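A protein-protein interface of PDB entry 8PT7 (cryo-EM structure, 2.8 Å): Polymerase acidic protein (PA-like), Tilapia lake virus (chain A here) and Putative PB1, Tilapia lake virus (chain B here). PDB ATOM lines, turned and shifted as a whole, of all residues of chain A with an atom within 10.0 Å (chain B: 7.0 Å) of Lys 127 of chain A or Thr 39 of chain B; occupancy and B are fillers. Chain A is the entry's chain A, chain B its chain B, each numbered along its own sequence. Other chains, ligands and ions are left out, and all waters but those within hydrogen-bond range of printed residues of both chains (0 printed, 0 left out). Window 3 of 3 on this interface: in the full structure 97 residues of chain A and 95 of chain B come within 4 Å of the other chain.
Lys 127 of chain A touches just these residues of chain B: Met 38, Thr 39, Gly 40 and Val 46. Thr 39 of chain B touches one residue of chain A. Printed residues of chain A within 4 Å of Gly 40 of chain B: Lys 127 (3.4 Å), Ser 128 (3.7 Å), Gly 129 (3.7 Å) and Pro 130 (3.7 Å). Of the printed residues of chain A, Val 46 of chain B touches Pro 126, Lys 127 and Ser 128. Of the printed residues of chain B, Pro 126 of chain A touches Met 38 and Val 46. Of the printed residues of chain B, Pro 124 of chain A touches Met 38. Of the printed residues of chain B, His 125 of chain A touches Met 38. Printed residues of chain A within 4 Å of Asn 44 of chain B: Ser 128 and Gly 129. Ala 34 of chain B touches none of the printed residues of chain A. Lys 41 of chain B touches none of the printed residues of chain A. The nearest residue of chain B that does not touch Lys 127 of chain A is Ile 37 of chain B (4.3 Å). The nearest residue of chain A that does not touch Thr 39 of chain B is Ser 128 of chain A (5.8 Å). The nearest printed residue of chain B that does not touch Pro 124 of chain A is Thr 39 of chain B (9.0 Å).
Among the printed residues, merely in contact across the chains: Gly 129 of chain A with Tyr 43 of chain B (3.4 Å), Lys 127 of chain A with Gly 40 of chain B (3.4 Å), Ser 128 of chain A with Val 46 of chain B (3.5 Å), Gly 129 of chain A with Asn 44 of chain B (3.6 Å), His 125 of chain A with Met 38 of chain B (3.6 Å), Lys 127 of chain A with Val 46 of chain B (3.6 Å), Pro 126 of chain A with Met 38 of chain B (3.6 Å), Lys 127 of chain A with Thr 39 of chain B (3.7 Å), Pro 126 of chain A with Val 46 of chain B (3.7 Å), Ser 128 of chain A with Gly 40 of chain B (3.7 Å), Ser 128 of chain A with Asn 44 of chain B (3.7 Å), Gly 129 of chain A with Gly 40 of chain B (3.7 Å), Pro 130 of chain A with Gly 40 of chain B (3.7 Å) and Pro 124 of chain A with Met 38 of chain B (3.8 Å).
N of Lys 127 of chain A lies within hydrogen-bond range of O of Met 38 of chain B, at 3.3 Å.
Of the 14 printed residues of chain B, 6 touch a printed residue of chain A. Printed residues of chain B that touch a printed residue of chain A: Met 38, Thr 39, Gly 40, Tyr 43, Asn 44 and Val 46. Hydrophobic or aromatic side chains of chain B within 4 Å of the printed part of chain A: Met 38 and Val 46. Of the 8 printed residues of chain A, 7 touch a printed residue of chain B. Printed residues of chain A that touch a printed residue of chain B: Pro 124, His 125, Pro 126, Lys 127, Ser 128, Gly 129 and Pro 130. Hydrophobic or aromatic side chains of chain A within 4 Å of the printed part of chain B: Pro 130. Among the printed residues, 15 pairs touch across the chains. Among the printed residues, no Asp or Glu carboxylate lies within 4 Å of a Lys or Arg side-chain nitrogen of the other chain.
The side-chain hydroxyl (OG1) of Thr 39 of chain B sits at hydrogen-bond distance from the backbone carbonyl oxygen (O) of Glu 36 of chain B. The side-chain amide oxygen (OD1) of Asn 44 of chain B is in hydrogen-bond range of the backbone NH (N) of Val 46 of chain B.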
ATOM      1  N   PRO A 124       6.277   2.313  23.406  1.00  0.00           N
ATOM      2  CA  PRO A 124       7.247   1.838  22.411  1.00  0.00           C
ATOM      3  C   PRO A 124       7.293   2.736  21.184  1.00  0.00           C
ATOM      4  O   PRO A 124       6.307   3.378  20.815  1.00  0.00           O
ATOM      5  CB  PRO A 124       6.737   0.437  22.053  1.00  0.00           C
ATOM      6  CG  PRO A 124       5.820   0.051  23.157  1.00  0.00           C
ATOM      7  CD  PRO A 124       5.225   1.319  23.669  1.00  0.00           C
ATOM      8  N   HIS A 125       8.462   2.774  20.551  1.00  0.00           N
ATOM      9  CA  HIS A 125       8.688   3.539  19.337  1.00  0.00           C
ATOM     10  C   HIS A 125       9.271   2.636  18.262  1.00  0.00           C
ATOM     11  O   HIS A 125       9.931   1.640  18.573  1.00  0.00           O
ATOM     12  CB  HIS A 125       9.644   4.714  19.587  1.00  0.00           C
ATOM     13  CG  HIS A 125       9.094   5.755  20.510  1.00  0.00           C
ATOM     14  ND1 HIS A 125       8.439   6.880  20.057  1.00  0.00           N
ATOM     15  CD2 HIS A 125       9.106   5.846  21.861  1.00  0.00           C
ATOM     16  CE1 HIS A 125       8.069   7.616  21.088  1.00  0.00           C
ATOM     17  NE2 HIS A 125       8.460   7.011  22.195  1.00  0.00           N
ATOM     18  N   PRO A 126       9.044   2.955  16.992  1.00  0.00           N
ATOM     19  CA  PRO A 126       9.560   2.110  15.912  1.00  0.00           C
ATOM     20  C   PRO A 126      11.049   2.320  15.683  1.00  0.00           C
ATOM     21  O   PRO A 126      11.639   3.326  16.080  1.00  0.00           O
ATOM     22  CB  PRO A 126       8.746   2.563  14.696  1.00  0.00           C
ATOM     23  CG  PRO A 126       8.420   3.982  14.978  1.00  0.00           C
ATOM     24  CD  PRO A 126       8.295   4.114  16.475  1.00  0.00           C
ATOM     25  N   LYS A 127      11.651   1.336  15.022  1.00  0.00           N
ATOM     26  CA  LYS A 127      13.056   1.373  14.647  1.00  0.00           C
ATOM     27  C   LYS A 127      13.172   1.650  13.156  1.00  0.00           C
ATOM     28  O   LYS A 127      12.385   1.133  12.357  1.00  0.00           O
ATOM     29  CB  LYS A 127      13.766   0.056  14.981  1.00  0.00           C
ATOM     30  CG  LYS A 127      13.343  -0.604  16.291  1.00  0.00           C
ATOM     31  CD  LYS A 127      14.382  -0.396  17.384  1.00  0.00           C
ATOM     32  CE  LYS A 127      14.216  -1.389  18.528  1.00  0.00           C
ATOM     33  NZ  LYS A 127      14.145  -2.804  18.067  1.00  0.00           N
ATOM     34  N   SER A 128      14.152   2.470  12.784  1.00  0.00           N
ATOM     35  CA  SER A 128      14.359   2.784  11.379  1.00  0.00           C
ATOM     36  C   SER A 128      14.600   1.507  10.586  1.00  0.00           C
ATOM     37  O   SER A 128      15.398   0.655  10.985  1.00  0.00           O
ATOM     38  CB  SER A 128      15.542   3.739  11.220  1.00  0.00           C
ATOM     39  OG  SER A 128      15.402   4.532  10.055  1.00  0.00           O
ATOM     40  N   GLY A 129      13.903   1.375   9.462  1.00  0.00           N
ATOM     41  CA  GLY A 129      14.008   0.198   8.637  1.00  0.00           C
ATOM     42  C   GLY A 129      15.185   0.266   7.689  1.00  0.00           C
ATOM     43  O   GLY A 129      15.835   1.305   7.539  1.00  0.00           O
ATOM     44  N   PRO A 130      15.483  -0.847   7.024  1.00  0.00           N
ATOM     45  CA  PRO A 130      16.597  -0.856   6.073  1.00  0.00           C
ATOM     46  C   PRO A 130      16.237  -0.131   4.787  1.00  0.00           C
ATOM     47  O   PRO A 130      15.096  -0.169   4.320  1.00  0.00           O
ATOM     48  CB  PRO A 130      16.842  -2.347   5.823  1.00  0.00           C
ATOM     49  CG  PRO A 130      15.532  -3.007   6.105  1.00  0.00           C
ATOM     50  CD  PRO A 130      14.751  -2.125   7.043  1.00  0.00           C
ATOM     51  N   LYS A 131      17.231   0.534   4.214  1.00  0.00           N
ATOM     52  CA  LYS A 131      17.029   1.256   2.966  1.00  0.00           C
ATOM     53  C   LYS A 131      16.941   0.260   1.815  1.00  0.00           C
ATOM     54  O   LYS A 131      17.895  -0.495   1.593  1.00  0.00           O
ATOM     55  CB  LYS A 131      18.168   2.238   2.728  1.00  0.00           C
ATOM     56  CG  LYS A 131      17.979   3.143   1.520  1.00  0.00           C
ATOM     57  CD  LYS A 131      17.411   4.494   1.919  1.00  0.00           C
ATOM     58  CE  LYS A 131      17.529   5.503   0.789  1.00  0.00           C
ATOM     59  NZ  LYS A 131      17.037   4.962  -0.508  1.00  0.00           N
ATOM     60  N   ARG B  33       2.059  -7.661  10.172  1.00  0.00           N
ATOM     61  CA  ARG B  33       2.881  -6.798   9.329  1.00  0.00           C
ATOM     62  C   ARG B  33       3.241  -5.511  10.056  1.00  0.00           C
ATOM     63  O   ARG B  33       4.381  -5.036   9.972  1.00  0.00           O
ATOM     64  CB  ARG B  33       2.153  -6.487   8.022  1.00  0.00           C
ATOM     65  CG  ARG B  33       2.032  -7.669   7.075  1.00  0.00           C
ATOM     66  CD  ARG B  33       3.395  -8.155   6.608  1.00  0.00           C
ATOM     67  NE  ARG B  33       3.865  -9.303   7.374  1.00  0.00           N
ATOM     68  CZ  ARG B  33       3.280 -10.494   7.380  1.00  0.00           C
ATOM     69  NH1 ARG B  33       2.203 -10.741   6.652  1.00  0.00           N
ATOM     70  NH2 ARG B  33       3.790 -11.463   8.135  1.00  0.00           N
ATOM     71  N   ALA B  34       2.277  -4.922  10.766  1.00  0.00           N
ATOM     72  CA  ALA B  34       2.558  -3.706  11.519  1.00  0.00           C
ATOM     73  C   ALA B  34       3.619  -3.955  12.582  1.00  0.00           C
ATOM     74  O   ALA B  34       4.533  -3.143  12.758  1.00  0.00           O
ATOM     75  CB  ALA B  34       1.275  -3.176  12.156  1.00  0.00           C
ATOM     76  N   SER B  35       3.520  -5.078  13.296  1.00  0.00           N
ATOM     77  CA  SER B  35       4.525  -5.398  14.305  1.00  0.00           C
ATOM     78  C   SER B  35       5.899  -5.593  13.673  1.00  0.00           C
ATOM     79  O   SER B  35       6.909  -5.101  14.194  1.00  0.00           O
ATOM     80  CB  SER B  35       4.111  -6.649  15.078  1.00  0.00           C
ATOM     81  OG  SER B  35       2.808  -6.507  15.615  1.00  0.00           O
ATOM     82  N   GLU B  36       5.956  -6.305  12.546  1.00  0.00           N
ATOM     83  CA  GLU B  36       7.234  -6.529  11.879  1.00  0.00           C
ATOM     84  C   GLU B  36       7.862  -5.211  11.449  1.00  0.00           C
ATOM     85  O   GLU B  36       9.070  -5.007  11.614  1.00  0.00           O
ATOM     86  CB  GLU B  36       7.044  -7.449  10.673  1.00  0.00           C
ATOM     87  CG  GLU B  36       7.495  -8.882  10.908  1.00  0.00           C
ATOM     88  CD  GLU B  36       6.618  -9.897  10.199  1.00  0.00           C
ATOM     89  OE1 GLU B  36       5.945  -9.523   9.214  1.00  0.00           O
ATOM     90  OE2 GLU B  36       6.600 -11.069  10.628  1.00  0.00           O
ATOM     91  N   ILE B  37       7.057  -4.302  10.895  1.00  0.00           N
ATOM     92  CA  ILE B  37       7.573  -2.986  10.533  1.00  0.00           C
ATOM     93  C   ILE B  37       8.026  -2.237  11.777  1.00  0.00           C
ATOM     94  O   ILE B  37       9.009  -1.487  11.739  1.00  0.00           O
ATOM     95  CB  ILE B  37       6.508  -2.194   9.750  1.00  0.00           C
ATOM     96  CG1 ILE B  37       6.330  -2.792   8.355  1.00  0.00           C
ATOM     97  CG2 ILE B  37       6.901  -0.729   9.653  1.00  0.00           C
ATOM     98  CD1 ILE B  37       5.038  -2.396   7.681  1.00  0.00           C
ATOM     99  N   MET B  38       7.322  -2.423  12.894  1.00  0.00           N
ATOM    100  CA  MET B  38       7.725  -1.787  14.142  1.00  0.00           C
ATOM    101  C   MET B  38       9.111  -2.250  14.568  1.00  0.00           C
ATOM    102  O   MET B  38       9.926  -1.446  15.036  1.00  0.00           O
ATOM    103  CB  MET B  38       6.699  -2.090  15.232  1.00  0.00           C
ATOM    104  CG  MET B  38       6.802  -1.195  16.450  1.00  0.00           C
ATOM    105  SD  MET B  38       5.531   0.080  16.476  1.00  0.00           S
ATOM    106  CE  MET B  38       6.077   1.058  17.869  1.00  0.00           C
ATOM    107  N   THR B  39       9.399  -3.545  14.416  1.00  0.00           N
ATOM    108  CA  THR B  39      10.730  -4.040  14.757  1.00  0.00           C
ATOM    109  C   THR B  39      11.809  -3.463  13.849  1.00  0.00           C
ATOM    110  O   THR B  39      12.995  -3.567  14.177  1.00  0.00           O
ATOM    111  CB  THR B  39      10.778  -5.569  14.692  1.00  0.00           C
ATOM    112  OG1 THR B  39      10.860  -5.993  13.325  1.00  0.00           O
ATOM    113  CG2 THR B  39       9.554  -6.186  15.350  1.00  0.00           C
ATOM    114  N   GLY B  40      11.431  -2.862  12.724  1.00  0.00           N
ATOM    115  CA  GLY B  40      12.390  -2.215  11.849  1.00  0.00           C
ATOM    116  C   GLY B  40      13.194  -3.175  10.999  1.00  0.00           C
ATOM    117  O   GLY B  40      14.351  -2.898  10.670  1.00  0.00           O
ATOM    118  N   LYS B  41      12.594  -4.309  10.634  1.00  0.00           N
ATOM    119  CA  LYS B  41      13.263  -5.314   9.823  1.00  0.00           C
ATOM    120  C   LYS B  41      12.685  -5.458   8.422  1.00  0.00           C
ATOM    121  O   LYS B  41      13.328  -6.090   7.577  1.00  0.00           O
ATOM    122  CB  LYS B  41      13.202  -6.686  10.516  1.00  0.00           C
ATOM    123  CG  LYS B  41      14.058  -6.847  11.782  1.00  0.00           C
ATOM    124  CD  LYS B  41      15.310  -5.977  11.797  1.00  0.00           C
ATOM    125  CE  LYS B  41      16.091  -6.157  13.088  1.00  0.00           C
ATOM    126  NZ  LYS B  41      17.297  -7.011  12.897  1.00  0.00           N
ATOM    127  N   SER B  42      11.509  -4.895   8.147  1.00  0.00           N
ATOM    128  CA  SER B  42      10.846  -5.067   6.862  1.00  0.00           C
ATOM    129  C   SER B  42      10.754  -3.767   6.075  1.00  0.00           C
ATOM    130  O   SER B  42      11.222  -3.701   4.934  1.00  0.00           O
ATOM    131  CB  SER B  42       9.448  -5.660   7.085  1.00  0.00           C
ATOM    132  OG  SER B  42       8.455  -4.652   7.042  1.00  0.00           O
ATOM    133  N   TYR B  43      10.164  -2.723   6.652  1.00  0.00           N
ATOM    134  CA  TYR B  43      10.037  -1.432   5.988  1.00  0.00           C
ATOM    135  C   TYR B  43      10.383  -0.344   6.997  1.00  0.00           C
ATOM    136  O   TYR B  43      10.781  -0.624   8.131  1.00  0.00           O
ATOM    137  CB  TYR B  43       8.631  -1.250   5.398  1.00  0.00           C
ATOM    138  CG  TYR B  43       8.278  -2.262   4.332  1.00  0.00           C
ATOM    139  CD1 TYR B  43       8.692  -2.088   3.020  1.00  0.00           C
ATOM    140  CD2 TYR B  43       7.525  -3.386   4.636  1.00  0.00           C
ATOM    141  CE1 TYR B  43       8.372  -3.008   2.043  1.00  0.00           C
ATOM    142  CE2 TYR B  43       7.201  -4.312   3.666  1.00  0.00           C
ATOM    143  CZ  TYR B  43       7.627  -4.118   2.371  1.00  0.00           C
ATOM    144  OH  TYR B  43       7.304  -5.038   1.401  1.00  0.00           O
ATOM    145  N   ASN B  44      10.224   0.909   6.581  1.00  0.00           N
ATOM    146  CA  ASN B  44      10.572   2.064   7.395  1.00  0.00           C
ATOM    147  C   ASN B  44       9.306   2.742   7.899  1.00  0.00           C
ATOM    148  O   ASN B  44       8.393   3.022   7.117  1.00  0.00           O
ATOM    149  CB  ASN B  44      11.414   3.061   6.599  1.00  0.00           C
ATOM    150  CG  ASN B  44      11.733   4.312   7.389  1.00  0.00           C
ATOM    151  OD1 ASN B  44      11.997   4.249   8.589  1.00  0.00           O
ATOM    152  ND2 ASN B  44      11.700   5.458   6.723  1.00  0.00           N
ATOM    153  N   ALA B  45       9.260   3.004   9.204  1.00  0.00           N
ATOM    154  CA  ALA B  45       8.153   3.722   9.823  1.00  0.00           C
ATOM    155  C   ALA B  45       8.617   4.962  10.576  1.00  0.00           C
ATOM    156  O   ALA B  45       7.800   5.613  11.237  1.00  0.00           O
ATOM    157  CB  ALA B  45       7.384   2.796  10.770  1.00  0.00           C
ATOM    158  N   VAL B  46       9.900   5.307  10.492  1.00  0.00           N
ATOM    159  CA  VAL B  46      10.462   6.453  11.198  1.00  0.00           C
ATOM    160  C   VAL B  46      10.554   7.620  10.228  1.00  0.00           C
ATOM    161  O   VAL B  46      11.233   7.530   9.198  1.00  0.00           O
ATOM    162  CB  VAL B  46      11.843   6.118  11.789  1.00  0.00           C
ATOM    163  CG1 VAL B  46      12.431   7.332  12.490  1.00  0.00           C
ATOM    164  CG2 VAL B  46      11.739   4.942  12.746  1.00  0.00           C
